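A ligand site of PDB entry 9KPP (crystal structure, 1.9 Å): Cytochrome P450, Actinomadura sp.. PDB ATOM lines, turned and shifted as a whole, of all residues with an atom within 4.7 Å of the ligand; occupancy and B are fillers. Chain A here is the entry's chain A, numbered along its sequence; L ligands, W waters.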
ATOM      1  N   LEU A  50     -27.976  -4.434   6.327  1.00  0.00           N
ATOM      2  CA  LEU A  50     -26.694  -4.107   5.712  1.00  0.00           C
ATOM      3  C   LEU A  50     -26.260  -5.143   4.669  1.00  0.00           C
ATOM      4  O   LEU A  50     -25.495  -4.803   3.755  1.00  0.00           O
ATOM      5  CB  LEU A  50     -25.621  -3.969   6.791  1.00  0.00           C
ATOM      6  CG  LEU A  50     -25.741  -2.778   7.761  1.00  0.00           C
ATOM      7  CD1 LEU A  50     -24.603  -2.801   8.798  1.00  0.00           C
ATOM      8  CD2 LEU A  50     -25.689  -1.470   6.990  1.00  0.00           C
ATOM      9  N   LEU A  81     -18.732   6.629  -3.554  1.00  0.00           N
ATOM     10  CA  LEU A  81     -18.907   5.190  -3.472  1.00  0.00           C
ATOM     11  C   LEU A  81     -20.089   4.801  -2.582  1.00  0.00           C
ATOM     12  O   LEU A  81     -20.789   3.831  -2.869  1.00  0.00           O
ATOM     13  CB  LEU A  81     -17.615   4.549  -2.966  1.00  0.00           C
ATOM     14  CG  LEU A  81     -17.617   3.024  -2.973  1.00  0.00           C
ATOM     15  CD1 LEU A  81     -17.612   2.480  -4.375  1.00  0.00           C
ATOM     16  CD2 LEU A  81     -16.365   2.576  -2.223  1.00  0.00           C
ATOM     17  N   THR A  82     -20.298   5.534  -1.483  1.00  0.00           N
ATOM     18  CA  THR A  82     -21.388   5.190  -0.568  1.00  0.00           C
ATOM     19  C   THR A  82     -22.760   5.421  -1.173  1.00  0.00           C
ATOM     20  O   THR A  82     -23.771   4.977  -0.591  1.00  0.00           O
ATOM     21  CB  THR A  82     -21.263   6.006   0.724  1.00  0.00           C
ATOM     22  OG1 THR A  82     -21.032   7.375   0.384  1.00  0.00           O
ATOM     23  CG2 THR A  82     -20.143   5.468   1.581  1.00  0.00           C
ATOM     24  N   HIS A  89     -20.999  -0.167  -8.181  1.00  0.00           N
ATOM     25  CA  HIS A  89     -20.360  -0.318  -6.874  1.00  0.00           C
ATOM     26  C   HIS A  89     -19.442  -1.526  -6.859  1.00  0.00           C
ATOM     27  O   HIS A  89     -18.345  -1.467  -6.284  1.00  0.00           O
ATOM     28  CB  HIS A  89     -21.422  -0.471  -5.776  1.00  0.00           C
ATOM     29  CG  HIS A  89     -20.838  -0.568  -4.402  1.00  0.00           C
ATOM     30  ND1 HIS A  89     -20.689  -1.768  -3.742  1.00  0.00           N
ATOM     31  CD2 HIS A  89     -20.335   0.376  -3.577  1.00  0.00           C
ATOM     32  CE1 HIS A  89     -20.122  -1.559  -2.561  1.00  0.00           C
ATOM     33  NE2 HIS A  89     -19.912  -0.259  -2.438  1.00  0.00           N
ATOM     34  N   LEU A  96     -10.885  -1.436  -4.921  1.00  0.00           N
ATOM     35  CA  LEU A  96     -10.445  -1.085  -3.571  1.00  0.00           C
ATOM     36  C   LEU A  96     -10.001  -2.308  -2.800  1.00  0.00           C
ATOM     37  O   LEU A  96      -9.052  -2.234  -2.002  1.00  0.00           O
ATOM     38  CB  LEU A  96     -11.548  -0.357  -2.825  1.00  0.00           C
ATOM     39  CG  LEU A  96     -11.652   1.135  -3.111  1.00  0.00           C
ATOM     40  CD1 LEU A  96     -12.754   1.765  -2.262  1.00  0.00           C
ATOM     41  CD2 LEU A  96     -10.303   1.770  -2.823  1.00  0.00           C
ATOM     42  N   PHE A 100      -6.468  -2.168  -0.950  1.00  0.00           N
ATOM     43  CA  PHE A 100      -6.406  -2.363   0.495  1.00  0.00           C
ATOM     44  C   PHE A 100      -6.224  -3.833   0.879  1.00  0.00           C
ATOM     45  O   PHE A 100      -6.644  -4.243   1.956  1.00  0.00           O
ATOM     46  CB  PHE A 100      -7.673  -1.788   1.148  1.00  0.00           C
ATOM     47  CG  PHE A 100      -7.677  -0.291   1.250  1.00  0.00           C
ATOM     48  CD1 PHE A 100      -7.113   0.342   2.345  1.00  0.00           C
ATOM     49  CD2 PHE A 100      -8.201   0.491   0.221  1.00  0.00           C
ATOM     50  CE1 PHE A 100      -7.094   1.730   2.443  1.00  0.00           C
ATOM     51  CE2 PHE A 100      -8.190   1.876   0.309  1.00  0.00           C
ATOM     52  CZ  PHE A 100      -7.627   2.511   1.414  1.00  0.00           C
ATOM     53  N   MET A 145      -3.056   9.505   6.807  1.00  0.00           N
ATOM     54  CA  MET A 145      -3.682   9.565   5.493  1.00  0.00           C
ATOM     55  C   MET A 145      -2.904  10.472   4.559  1.00  0.00           C
ATOM     56  O   MET A 145      -2.769  10.175   3.364  1.00  0.00           O
ATOM     57  CB  MET A 145      -5.130  10.023   5.611  1.00  0.00           C
ATOM     58  CG  MET A 145      -5.946   8.996   6.374  1.00  0.00           C
ATOM     59  SD  MET A 145      -6.059   7.382   5.613  1.00  0.00           S
ATOM     60  CE  MET A 145      -6.015   7.673   3.834  1.00  0.00           C
ATOM     61  N   LEU A 225     -12.952   9.481  -4.721  1.00  0.00           N
ATOM     62  CA  LEU A 225     -12.463   8.425  -3.803  1.00  0.00           C
ATOM     63  C   LEU A 225     -11.266   8.944  -3.001  1.00  0.00           C
ATOM     64  O   LEU A 225     -11.238   8.733  -1.792  1.00  0.00           O
ATOM     65  CB  LEU A 225     -12.061   7.186  -4.610  1.00  0.00           C
ATOM     66  CG  LEU A 225     -11.986   5.858  -3.861  1.00  0.00           C
ATOM     67  CD1 LEU A 225     -13.132   5.669  -2.882  1.00  0.00           C
ATOM     68  CD2 LEU A 225     -11.980   4.738  -4.885  1.00  0.00           C
ATOM     69  N   MET A 228     -12.597  11.230  -0.331  1.00  0.00           N
ATOM     70  CA  MET A 228     -13.380  10.465   0.676  1.00  0.00           C
ATOM     71  C   MET A 228     -12.441   9.638   1.569  1.00  0.00           C
ATOM     72  O   MET A 228     -12.648   9.604   2.777  1.00  0.00           O
ATOM     73  CB  MET A 228     -14.398   9.537   0.000  1.00  0.00           C
ATOM     74  CG  MET A 228     -15.320   8.908   1.003  1.00  0.00           C
ATOM     75  SD  MET A 228     -14.813   7.181   1.115  1.00  0.00           S
ATOM     76  CE  MET A 228     -16.005   6.672  -0.125  1.00  0.00           C
ATOM     77  N   LEU A 229     -11.455   9.007   0.949  1.00  0.00           N
ATOM     78  CA  LEU A 229     -10.560   8.130   1.741  1.00  0.00           C
ATOM     79  C   LEU A 229      -9.826   8.988   2.788  1.00  0.00           C
ATOM     80  O   LEU A 229      -9.689   8.534   3.920  1.00  0.00           O
ATOM     81  CB  LEU A 229      -9.591   7.449   0.780  1.00  0.00           C
ATOM     82  CG  LEU A 229     -10.149   6.260  -0.009  1.00  0.00           C
ATOM     83  CD1 LEU A 229      -9.159   5.803  -1.057  1.00  0.00           C
ATOM     84  CD2 LEU A 229     -10.560   5.114   0.890  1.00  0.00           C
ATOM     85  N   ALA A 232     -12.641  10.034   5.516  1.00  0.00           N
ATOM     86  CA  ALA A 232     -13.064   8.905   6.330  1.00  0.00           C
ATOM     87  C   ALA A 232     -11.930   8.401   7.205  1.00  0.00           C
ATOM     88  O   ALA A 232     -12.104   8.187   8.410  1.00  0.00           O
ATOM     89  CB  ALA A 232     -13.599   7.785   5.433  1.00  0.00           C
ATOM     90  N   GLY A 233     -10.746   8.201   6.605  1.00  0.00           N
ATOM     91  CA  GLY A 233      -9.620   7.699   7.357  1.00  0.00           C
ATOM     92  C   GLY A 233      -9.196   8.616   8.480  1.00  0.00           C
ATOM     93  O   GLY A 233      -8.604   8.149   9.456  1.00  0.00           O
ATOM     94  N   THR A 236     -13.297   9.486  11.316  1.00  0.00           N
ATOM     95  CA  THR A 236     -13.900   8.343  12.028  1.00  0.00           C
ATOM     96  C   THR A 236     -12.871   7.743  12.953  1.00  0.00           C
ATOM     97  O   THR A 236     -13.181   7.510  14.123  1.00  0.00           O
ATOM     98  CB  THR A 236     -14.492   7.372  11.013  1.00  0.00           C
ATOM     99  OG1 THR A 236     -13.390   6.678  10.426  1.00  0.00           O
ATOM    100  CG2 THR A 236     -15.253   8.088   9.913  1.00  0.00           C
ATOM    101  N   THR A 237     -11.663   7.526  12.429  1.00  0.00           N
ATOM    102  CA  THR A 237     -10.591   6.925  13.238  1.00  0.00           C
ATOM    103  C   THR A 237     -10.315   7.818  14.448  1.00  0.00           C
ATOM    104  O   THR A 237     -10.251   7.313  15.567  1.00  0.00           O
ATOM    105  CB  THR A 237      -9.354   6.692  12.365  1.00  0.00           C
ATOM    106  OG1 THR A 237      -9.796   6.085  11.149  1.00  0.00           O
ATOM    107  CG2 THR A 237      -8.334   5.803  13.052  1.00  0.00           C
ATOM    108  N   VAL A 240     -13.069   7.440  17.122  1.00  0.00           N
ATOM    109  CA  VAL A 240     -12.986   6.159  17.836  1.00  0.00           C
ATOM    110  C   VAL A 240     -11.785   6.136  18.759  1.00  0.00           C
ATOM    111  O   VAL A 240     -11.852   5.618  19.884  1.00  0.00           O
ATOM    112  CB  VAL A 240     -12.927   4.988  16.846  1.00  0.00           C
ATOM    113  CG1 VAL A 240     -12.550   3.691  17.577  1.00  0.00           C
ATOM    114  CG2 VAL A 240     -14.260   4.807  16.166  1.00  0.00           C
ATOM    115  N   LEU A 272     -13.950  -0.489  19.404  1.00  0.00           N
ATOM    116  CA  LEU A 272     -14.796  -0.323  18.222  1.00  0.00           C
ATOM    117  C   LEU A 272     -16.268  -0.597  18.563  1.00  0.00           C
ATOM    118  O   LEU A 272     -17.152   0.135  18.106  1.00  0.00           O
ATOM    119  CB  LEU A 272     -14.328  -1.236  17.087  1.00  0.00           C
ATOM    120  CG  LEU A 272     -13.082  -0.694  16.369  1.00  0.00           C
ATOM    121  CD1 LEU A 272     -12.309  -1.834  15.686  1.00  0.00           C
ATOM    122  CD2 LEU A 272     -13.490   0.376  15.348  1.00  0.00           C
ATOM    123  N   PRO A 277     -18.904   5.391  16.828  1.00  0.00           N
ATOM    124  CA  PRO A 277     -19.153   6.821  16.929  1.00  0.00           C
ATOM    125  C   PRO A 277     -20.373   7.381  16.229  1.00  0.00           C
ATOM    126  O   PRO A 277     -20.600   8.601  16.267  1.00  0.00           O
ATOM    127  CB  PRO A 277     -17.852   7.339  16.291  1.00  0.00           C
ATOM    128  CG  PRO A 277     -17.594   6.422  15.141  1.00  0.00           C
ATOM    129  CD  PRO A 277     -18.022   5.080  15.677  1.00  0.00           C
ATOM    130  N   LEU A 282     -26.054   5.492   7.147  1.00  0.00           N
ATOM    131  CA  LEU A 282     -26.651   5.800   5.835  1.00  0.00           C
ATOM    132  C   LEU A 282     -27.932   4.976   5.600  1.00  0.00           C
ATOM    133  O   LEU A 282     -27.944   3.775   5.875  1.00  0.00           O
ATOM    134  CB  LEU A 282     -25.592   5.540   4.770  1.00  0.00           C
ATOM    135  CG  LEU A 282     -24.366   6.465   4.833  1.00  0.00           C
ATOM    136  CD1 LEU A 282     -23.454   6.175   3.662  1.00  0.00           C
ATOM    137  CD2 LEU A 282     -24.819   7.909   4.835  1.00  0.00           C
ATOM    138  N   ARG A 284     -31.004   2.896   3.965  1.00  0.00           N
ATOM    139  CA  ARG A 284     -31.126   1.841   2.927  1.00  0.00           C
ATOM    140  C   ARG A 284     -32.582   1.853   2.411  1.00  0.00           C
ATOM    141  O   ARG A 284     -33.504   1.879   3.228  1.00  0.00           O
ATOM    142  CB  ARG A 284     -30.793   0.435   3.433  1.00  0.00           C
ATOM    143  CG  ARG A 284     -29.439   0.220   4.095  1.00  0.00           C
ATOM    144  CD  ARG A 284     -28.256   0.886   3.445  1.00  0.00           C
ATOM    145  NE  ARG A 284     -27.020   0.156   3.722  1.00  0.00           N
ATOM    146  CZ  ARG A 284     -25.898   0.697   4.166  1.00  0.00           C
ATOM    147  NH1 ARG A 284     -25.950   1.807   4.870  1.00  0.00           N
ATOM    148  NH2 ARG A 284     -24.745   0.134   3.893  1.00  0.00           N
ATOM    149  N   MET A 307     -25.821   0.902  13.779  1.00  0.00           N
ATOM    150  CA  MET A 307     -24.760  -0.056  14.155  1.00  0.00           C
ATOM    151  C   MET A 307     -24.446   0.111  15.665  1.00  0.00           C
ATOM    152  O   MET A 307     -24.189  -0.903  16.335  1.00  0.00           O
ATOM    153  CB  MET A 307     -23.551   0.148  13.232  1.00  0.00           C
ATOM    154  CG  MET A 307     -23.897   0.043  11.760  1.00  0.00           C
ATOM    155  SD  MET A 307     -22.596   0.648  10.654  1.00  0.00           S
ATOM    156  CE  MET A 307     -23.616   1.226   9.286  1.00  0.00           C
ATOM    157  N   THR A 334     -19.261  -2.081  13.702  1.00  0.00           N
ATOM    158  CA  THR A 334     -18.756  -0.704  13.638  1.00  0.00           C
ATOM    159  C   THR A 334     -18.142  -0.393  12.282  1.00  0.00           C
ATOM    160  O   THR A 334     -18.157   0.752  11.849  1.00  0.00           O
ATOM    161  CB  THR A 334     -17.762  -0.466  14.766  1.00  0.00           C
ATOM    162  OG1 THR A 334     -18.417  -0.757  16.013  1.00  0.00           O
ATOM    163  CG2 THR A 334     -17.265   1.009  14.760  1.00  0.00           C
ATOM    164  N   PHE A 335     -17.694  -1.421  11.566  1.00  0.00           N
ATOM    165  CA  PHE A 335     -17.261  -1.267  10.177  1.00  0.00           C
ATOM    166  C   PHE A 335     -18.368  -1.619   9.192  1.00  0.00           C
ATOM    167  O   PHE A 335     -18.102  -1.731   7.980  1.00  0.00           O
ATOM    168  CB  PHE A 335     -16.031  -2.142   9.934  1.00  0.00           C
ATOM    169  CG  PHE A 335     -14.787  -1.638  10.601  1.00  0.00           C
ATOM    170  CD1 PHE A 335     -14.343  -0.325  10.416  1.00  0.00           C
ATOM    171  CD2 PHE A 335     -14.053  -2.476  11.430  1.00  0.00           C
ATOM    172  CE1 PHE A 335     -13.171   0.136  11.050  1.00  0.00           C
ATOM    173  CE2 PHE A 335     -12.890  -2.026  12.064  1.00  0.00           C
ATOM    174  CZ  PHE A 335     -12.455  -0.706  11.866  1.00  0.00           C
ATOM    175  N   GLY A 336     -19.605  -1.777   9.669  1.00  0.00           N
ATOM    176  CA  GLY A 336     -20.709  -2.173   8.802  1.00  0.00           C
ATOM    177  C   GLY A 336     -20.671  -3.650   8.458  1.00  0.00           C
ATOM    178  O   GLY A 336     -20.121  -4.480   9.202  1.00  0.00           O
ATOM    179  N   ALA A 339     -22.225  -5.173   1.291  1.00  0.00           N
ATOM    180  CA  ALA A 339     -21.570  -4.563   0.145  1.00  0.00           C
ATOM    181  C   ALA A 339     -20.717  -3.358   0.533  1.00  0.00           C
ATOM    182  O   ALA A 339     -19.618  -3.164  -0.017  1.00  0.00           O
ATOM    183  CB  ALA A 339     -22.616  -4.134  -0.892  1.00  0.00           C
ATOM    184  N   HIS A 340     -21.204  -2.519   1.451  1.00  0.00           N
ATOM    185  CA  HIS A 340     -20.490  -1.288   1.777  1.00  0.00           C
ATOM    186  C   HIS A 340     -19.616  -1.411   3.029  1.00  0.00           C
ATOM    187  O   HIS A 340     -19.260  -0.384   3.621  1.00  0.00           O
ATOM    188  CB  HIS A 340     -21.471  -0.124   1.923  1.00  0.00           C
ATOM    189  CG  HIS A 340     -22.199   0.225   0.651  1.00  0.00           C
ATOM    190  ND1 HIS A 340     -21.788   1.237  -0.190  1.00  0.00           N
ATOM    191  CD2 HIS A 340     -23.296  -0.321   0.078  1.00  0.00           C
ATOM    192  CE1 HIS A 340     -22.607   1.305  -1.235  1.00  0.00           C
ATOM    193  NE2 HIS A 340     -23.530   0.372  -1.086  1.00  0.00           N
ATOM    194  N   TYR A 341     -19.254  -2.626   3.422  1.00  0.00           N
ATOM    195  CA  TYR A 341     -18.311  -2.845   4.522  1.00  0.00           C
ATOM    196  C   TYR A 341     -17.095  -1.947   4.333  1.00  0.00           C
ATOM    197  O   TYR A 341     -16.566  -1.831   3.236  1.00  0.00           O
ATOM    198  CB  TYR A 341     -17.880  -4.316   4.561  1.00  0.00           C
ATOM    199  CG  TYR A 341     -16.987  -4.690   5.745  1.00  0.00           C
ATOM    200  CD1 TYR A 341     -17.512  -4.831   7.019  1.00  0.00           C
ATOM    201  CD2 TYR A 341     -15.633  -4.914   5.565  1.00  0.00           C
ATOM    202  CE1 TYR A 341     -16.702  -5.197   8.111  1.00  0.00           C
ATOM    203  CE2 TYR A 341     -14.802  -5.270   6.638  1.00  0.00           C
ATOM    204  CZ  TYR A 341     -15.348  -5.403   7.908  1.00  0.00           C
ATOM    205  OH  TYR A 341     -14.534  -5.765   8.959  1.00  0.00           O
ATOM    206  N   CYS A 342     -16.663  -1.308   5.421  1.00  0.00           N
ATOM    207  CA  CYS A 342     -15.528  -0.395   5.403  1.00  0.00           C
ATOM    208  C   CYS A 342     -14.371  -0.924   4.578  1.00  0.00           C
ATOM    209  O   CYS A 342     -13.783  -1.950   4.915  1.00  0.00           O
ATOM    210  CB  CYS A 342     -15.065  -0.141   6.830  1.00  0.00           C
ATOM    211  SG  CYS A 342     -13.718   1.058   6.872  1.00  0.00           S
ATOM    212  N   ALA A 343     -14.034  -0.194   3.520  1.00  0.00           N
ATOM    213  CA  ALA A 343     -12.922  -0.580   2.671  1.00  0.00           C
ATOM    214  C   ALA A 343     -11.579  -0.406   3.363  1.00  0.00           C
ATOM    215  O   ALA A 343     -10.595  -1.037   2.956  1.00  0.00           O
ATOM    216  CB  ALA A 343     -12.945   0.239   1.375  1.00  0.00           C
ATOM    217  N   GLY A 344     -11.500   0.448   4.380  1.00  0.00           N
ATOM    218  CA  GLY A 344     -10.243   0.653   5.078  1.00  0.00           C
ATOM    219  C   GLY A 344     -10.161  -0.030   6.425  1.00  0.00           C
ATOM    220  O   GLY A 344      -9.274   0.302   7.223  1.00  0.00           O
ATOM    221  N   LEU A 347      -6.704  -1.202   7.683  1.00  0.00           N
ATOM    222  CA  LEU A 347      -5.826  -0.100   8.046  1.00  0.00           C
ATOM    223  C   LEU A 347      -6.280   0.544   9.349  1.00  0.00           C
ATOM    224  O   LEU A 347      -5.448   0.849  10.215  1.00  0.00           O
ATOM    225  CB  LEU A 347      -5.787   0.955   6.930  1.00  0.00           C
ATOM    226  CG  LEU A 347      -5.030   2.235   7.275  1.00  0.00           C
ATOM    227  CD1 LEU A 347      -3.553   1.953   7.524  1.00  0.00           C
ATOM    228  CD2 LEU A 347      -5.223   3.275   6.163  1.00  0.00           C
ATOM    229  N   ALA A 348      -7.600   0.757   9.504  1.00  0.00           N
ATOM    230  CA  ALA A 348      -8.104   1.412  10.709  1.00  0.00           C
ATOM    231  C   ALA A 348      -7.829   0.572  11.948  1.00  0.00           C
ATOM    232  O   ALA A 348      -7.386   1.092  12.982  1.00  0.00           O
ATOM    233  CB  ALA A 348      -9.604   1.696  10.569  1.00  0.00           C
ATOM    234  N   LEU A 352      -5.404   1.717  15.218  1.00  0.00           N
ATOM    235  CA  LEU A 352      -5.830   1.655  16.616  1.00  0.00           C
ATOM    236  C   LEU A 352      -4.923   0.752  17.423  1.00  0.00           C
ATOM    237  O   LEU A 352      -4.518   1.096  18.536  1.00  0.00           O
ATOM    238  CB  LEU A 352      -7.277   1.163  16.694  1.00  0.00           C
ATOM    239  CG  LEU A 352      -8.304   2.057  15.975  1.00  0.00           C
ATOM    240  CD1 LEU A 352      -9.645   1.349  15.880  1.00  0.00           C
ATOM    241  CD2 LEU A 352      -8.444   3.408  16.657  1.00  0.00           C
HETATM  242  C1  LIG L   1     -17.341   2.661   4.777  1.00  0.00           C
HETATM  243  C2  LIG L   1     -16.625   2.825   9.527  1.00  0.00           C
HETATM  244  C3  LIG L   1     -12.001   4.027   8.866  1.00  0.00           C
HETATM  245  C4  LIG L   1     -12.768   4.040   4.107  1.00  0.00           C
HETATM  246  C5  LIG L   1     -17.544   2.557   6.126  1.00  0.00           C
HETATM  247  C6  LIG L   1     -18.772   2.115   6.753  1.00  0.00           C
HETATM  248  C7  LIG L   1     -18.580   2.175   8.099  1.00  0.00           C
HETATM  249  C8  LIG L   1     -17.219   2.636   8.299  1.00  0.00           C
HETATM  250  C9  LIG L   1     -19.586   1.851   9.165  1.00  0.00           C
HETATM  251  C10 LIG L   1     -20.009   1.684   6.026  1.00  0.00           C
HETATM  252  C11 LIG L   1     -21.129   2.731   6.098  1.00  0.00           C
HETATM  253  C12 LIG L   1     -22.459   2.174   5.630  1.00  0.00           C
HETATM  254  O1  LIG L   1     -23.477   2.862   5.822  1.00  0.00           O
HETATM  255  O2  LIG L   1     -22.475   1.059   5.091  1.00  0.00           O
HETATM  256  C13 LIG L   1     -15.331   3.196   9.791  1.00  0.00           C
HETATM  257  C14 LIG L   1     -14.732   3.267  11.115  1.00  0.00           C
HETATM  258  C15 LIG L   1     -13.392   3.686  10.892  1.00  0.00           C
HETATM  259  C16 LIG L   1     -13.204   3.774   9.512  1.00  0.00           C
HETATM  260  C17 LIG L   1     -15.413   2.971  12.420  1.00  0.00           C
HETATM  261  C18 LIG L   1     -12.351   3.916  11.783  1.00  0.00           C
HETATM  262  C19 LIG L   1     -12.277   3.479  13.016  1.00  0.00           C
HETATM  263  C20 LIG L   1     -11.751   4.085   7.508  1.00  0.00           C
HETATM  264  C21 LIG L   1     -10.436   4.232   6.890  1.00  0.00           C
HETATM  265  C22 LIG L   1     -10.712   4.319   5.493  1.00  0.00           C
HETATM  266  C23 LIG L   1     -12.087   4.114   5.320  1.00  0.00           C
HETATM  267  C24 LIG L   1      -9.106   4.263   7.588  1.00  0.00           C
HETATM  268  C25 LIG L   1      -9.853   4.533   4.414  1.00  0.00           C
HETATM  269  C26 LIG L   1      -8.562   4.736   4.425  1.00  0.00           C
HETATM  270  C27 LIG L   1     -14.084   3.732   3.883  1.00  0.00           C
HETATM  271  C28 LIG L   1     -14.753   3.800   2.583  1.00  0.00           C
HETATM  272  C29 LIG L   1     -16.027   3.364   2.776  1.00  0.00           C
HETATM  273  C30 LIG L   1     -16.186   3.099   4.182  1.00  0.00           C
HETATM  274  C31 LIG L   1     -14.132   4.233   1.294  1.00  0.00           C
HETATM  275  C32 LIG L   1     -17.109   3.180   1.742  1.00  0.00           C
HETATM  276  C33 LIG L   1     -17.263   1.716   1.282  1.00  0.00           C
HETATM  277  C34 LIG L   1     -18.419   1.494   0.314  1.00  0.00           C
HETATM  278  O3  LIG L   1     -19.381   2.269   0.360  1.00  0.00           O
HETATM  279  O4  LIG L   1     -18.359   0.537  -0.459  1.00  0.00           O
HETATM  280  N1  LIG L   1     -16.610   2.856   7.087  1.00  0.00           N
HETATM  281  N2  LIG L   1     -14.405   3.570   8.851  1.00  0.00           N
HETATM  282  N3  LIG L   1     -12.699   3.987   6.540  1.00  0.00           N
HETATM  283  N4  LIG L   1     -14.992   3.345   4.857  1.00  0.00           N
HETATM  284 FE1  LIG L   1     -14.596   3.216   6.791  1.00  0.00          FE
HETATM  285  O   HOH W   1     -21.784  -1.557   5.451  1.00  0.00           O
HETATM  286  O   HOH W   2     -15.173   5.766   7.235  1.00  0.00           O
HETATM  287  O   HOH W   3     -23.286   4.793   7.751  1.00  0.00           O
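N of Cys 342 lies within hydrogen-bond range of O of Phe 335, 3.0 Å away. SG of Cys 342 lies close to N of Gly 344. A ring nitrogen (NE2) of His 89 is in hydrogen-bond range of a ring nitrogen (ND1) of His 340, at 3.3 Å. The guanidinium group of Arg 284 is in hydrogen-bond range of the backbone carbonyl oxygen of Leu 282. OG1 of Thr 236 lies within hydrogen-bond range of O of Ala 232 (2.8 Å). The side-chain hydroxyl of Thr 334 lies within hydrogen-bond range of the backbone carbonyl oxygen of Leu 272 (2.6 Å). OG1 of Thr 237 lies within hydrogen-bond range of O of Gly 233 (2.9 Å).
Water W1 lies within hydrogen-bond range of an oxygen (O2) of the ligand, the backbone carbonyl oxygen of His 340 and the backbone NH of Tyr 341. Water W3 lies within hydrogen-bond range of O1 of the ligand (2.7 Å) and N of Leu 282 (2.9 Å).
An iron atom (FE1) of the ligand is bound by the side-chain sulfur (SG) of Cys 342. NE2 of His 89 lies within hydrogen-bond range of O4 of the ligand, 2.6 Å away. A ring nitrogen (ND1) of His 340 is in hydrogen-bond range of an oxygen (O3) of the ligand (2.7 Å). NH2 of Arg 284 is in salt-bridge range of O2 of the ligand, 2.7 Å away.
Leu 81 touches the ligand. CG2 of Thr 82 touches O3 of the ligand, at 3.5 Å. CZ of Phe 100 touches C26 of the ligand, at 3.9 Å. Met 145 touches the ligand. Met 228 touches the ligand. Leu 229 touches the ligand (CD2 to C25, 3.6 Å). Ala 232 touches the ligand (CB to C23, 3.97 Å). Gly 233 touches the ligand (CA to C24, 3.5 Å). Thr 236 touches the ligand (OG1 to C15, 3.0 Å). Thr 237 touches the ligand. Val 240 touches the ligand (CG2 to C19, 3.95 Å). CB of Leu 282 touches O1 of the ligand (3.6 Å). Met 307 touches the ligand (SD to C9, 3.6 Å). Thr 334 touches the ligand (O to C9, 3.2 Å). CE1 of Phe 335 touches C14 of the ligand, 3.5 Å away. N of Gly 336 touches C9 of the ligand, at 3.7 Å. Ala 339 touches the ligand (O to O4, 3.9 Å). Ala 343 touches the ligand (N to N4, 3.9 Å). Gly 344 touches the ligand (CA to C22, 3.7 Å). Ala 348 touches the ligand (CB to C18, 3.7 Å). Hydrophobic or aromatic side chains that line the ligand: Leu 81, His 89, Phe 100, Met 145, Met 228, Leu 229, Ala 232, Val 240, Leu 282, Met 307, Phe 335, His 340 and Ala 348. Within 4 Å of the ligand: Leu 81, Thr 82, His 89, Phe 100, Met 145, Met 228, Leu 229, Ala 232, Gly 233, Thr 236, Thr 237, Val 240, Leu 282, Arg 284, Met 307, Thr 334, Phe 335, Gly 336, Ala 339, His 340, Cys 342, Ala 343, Gly 344 and Ala 348.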
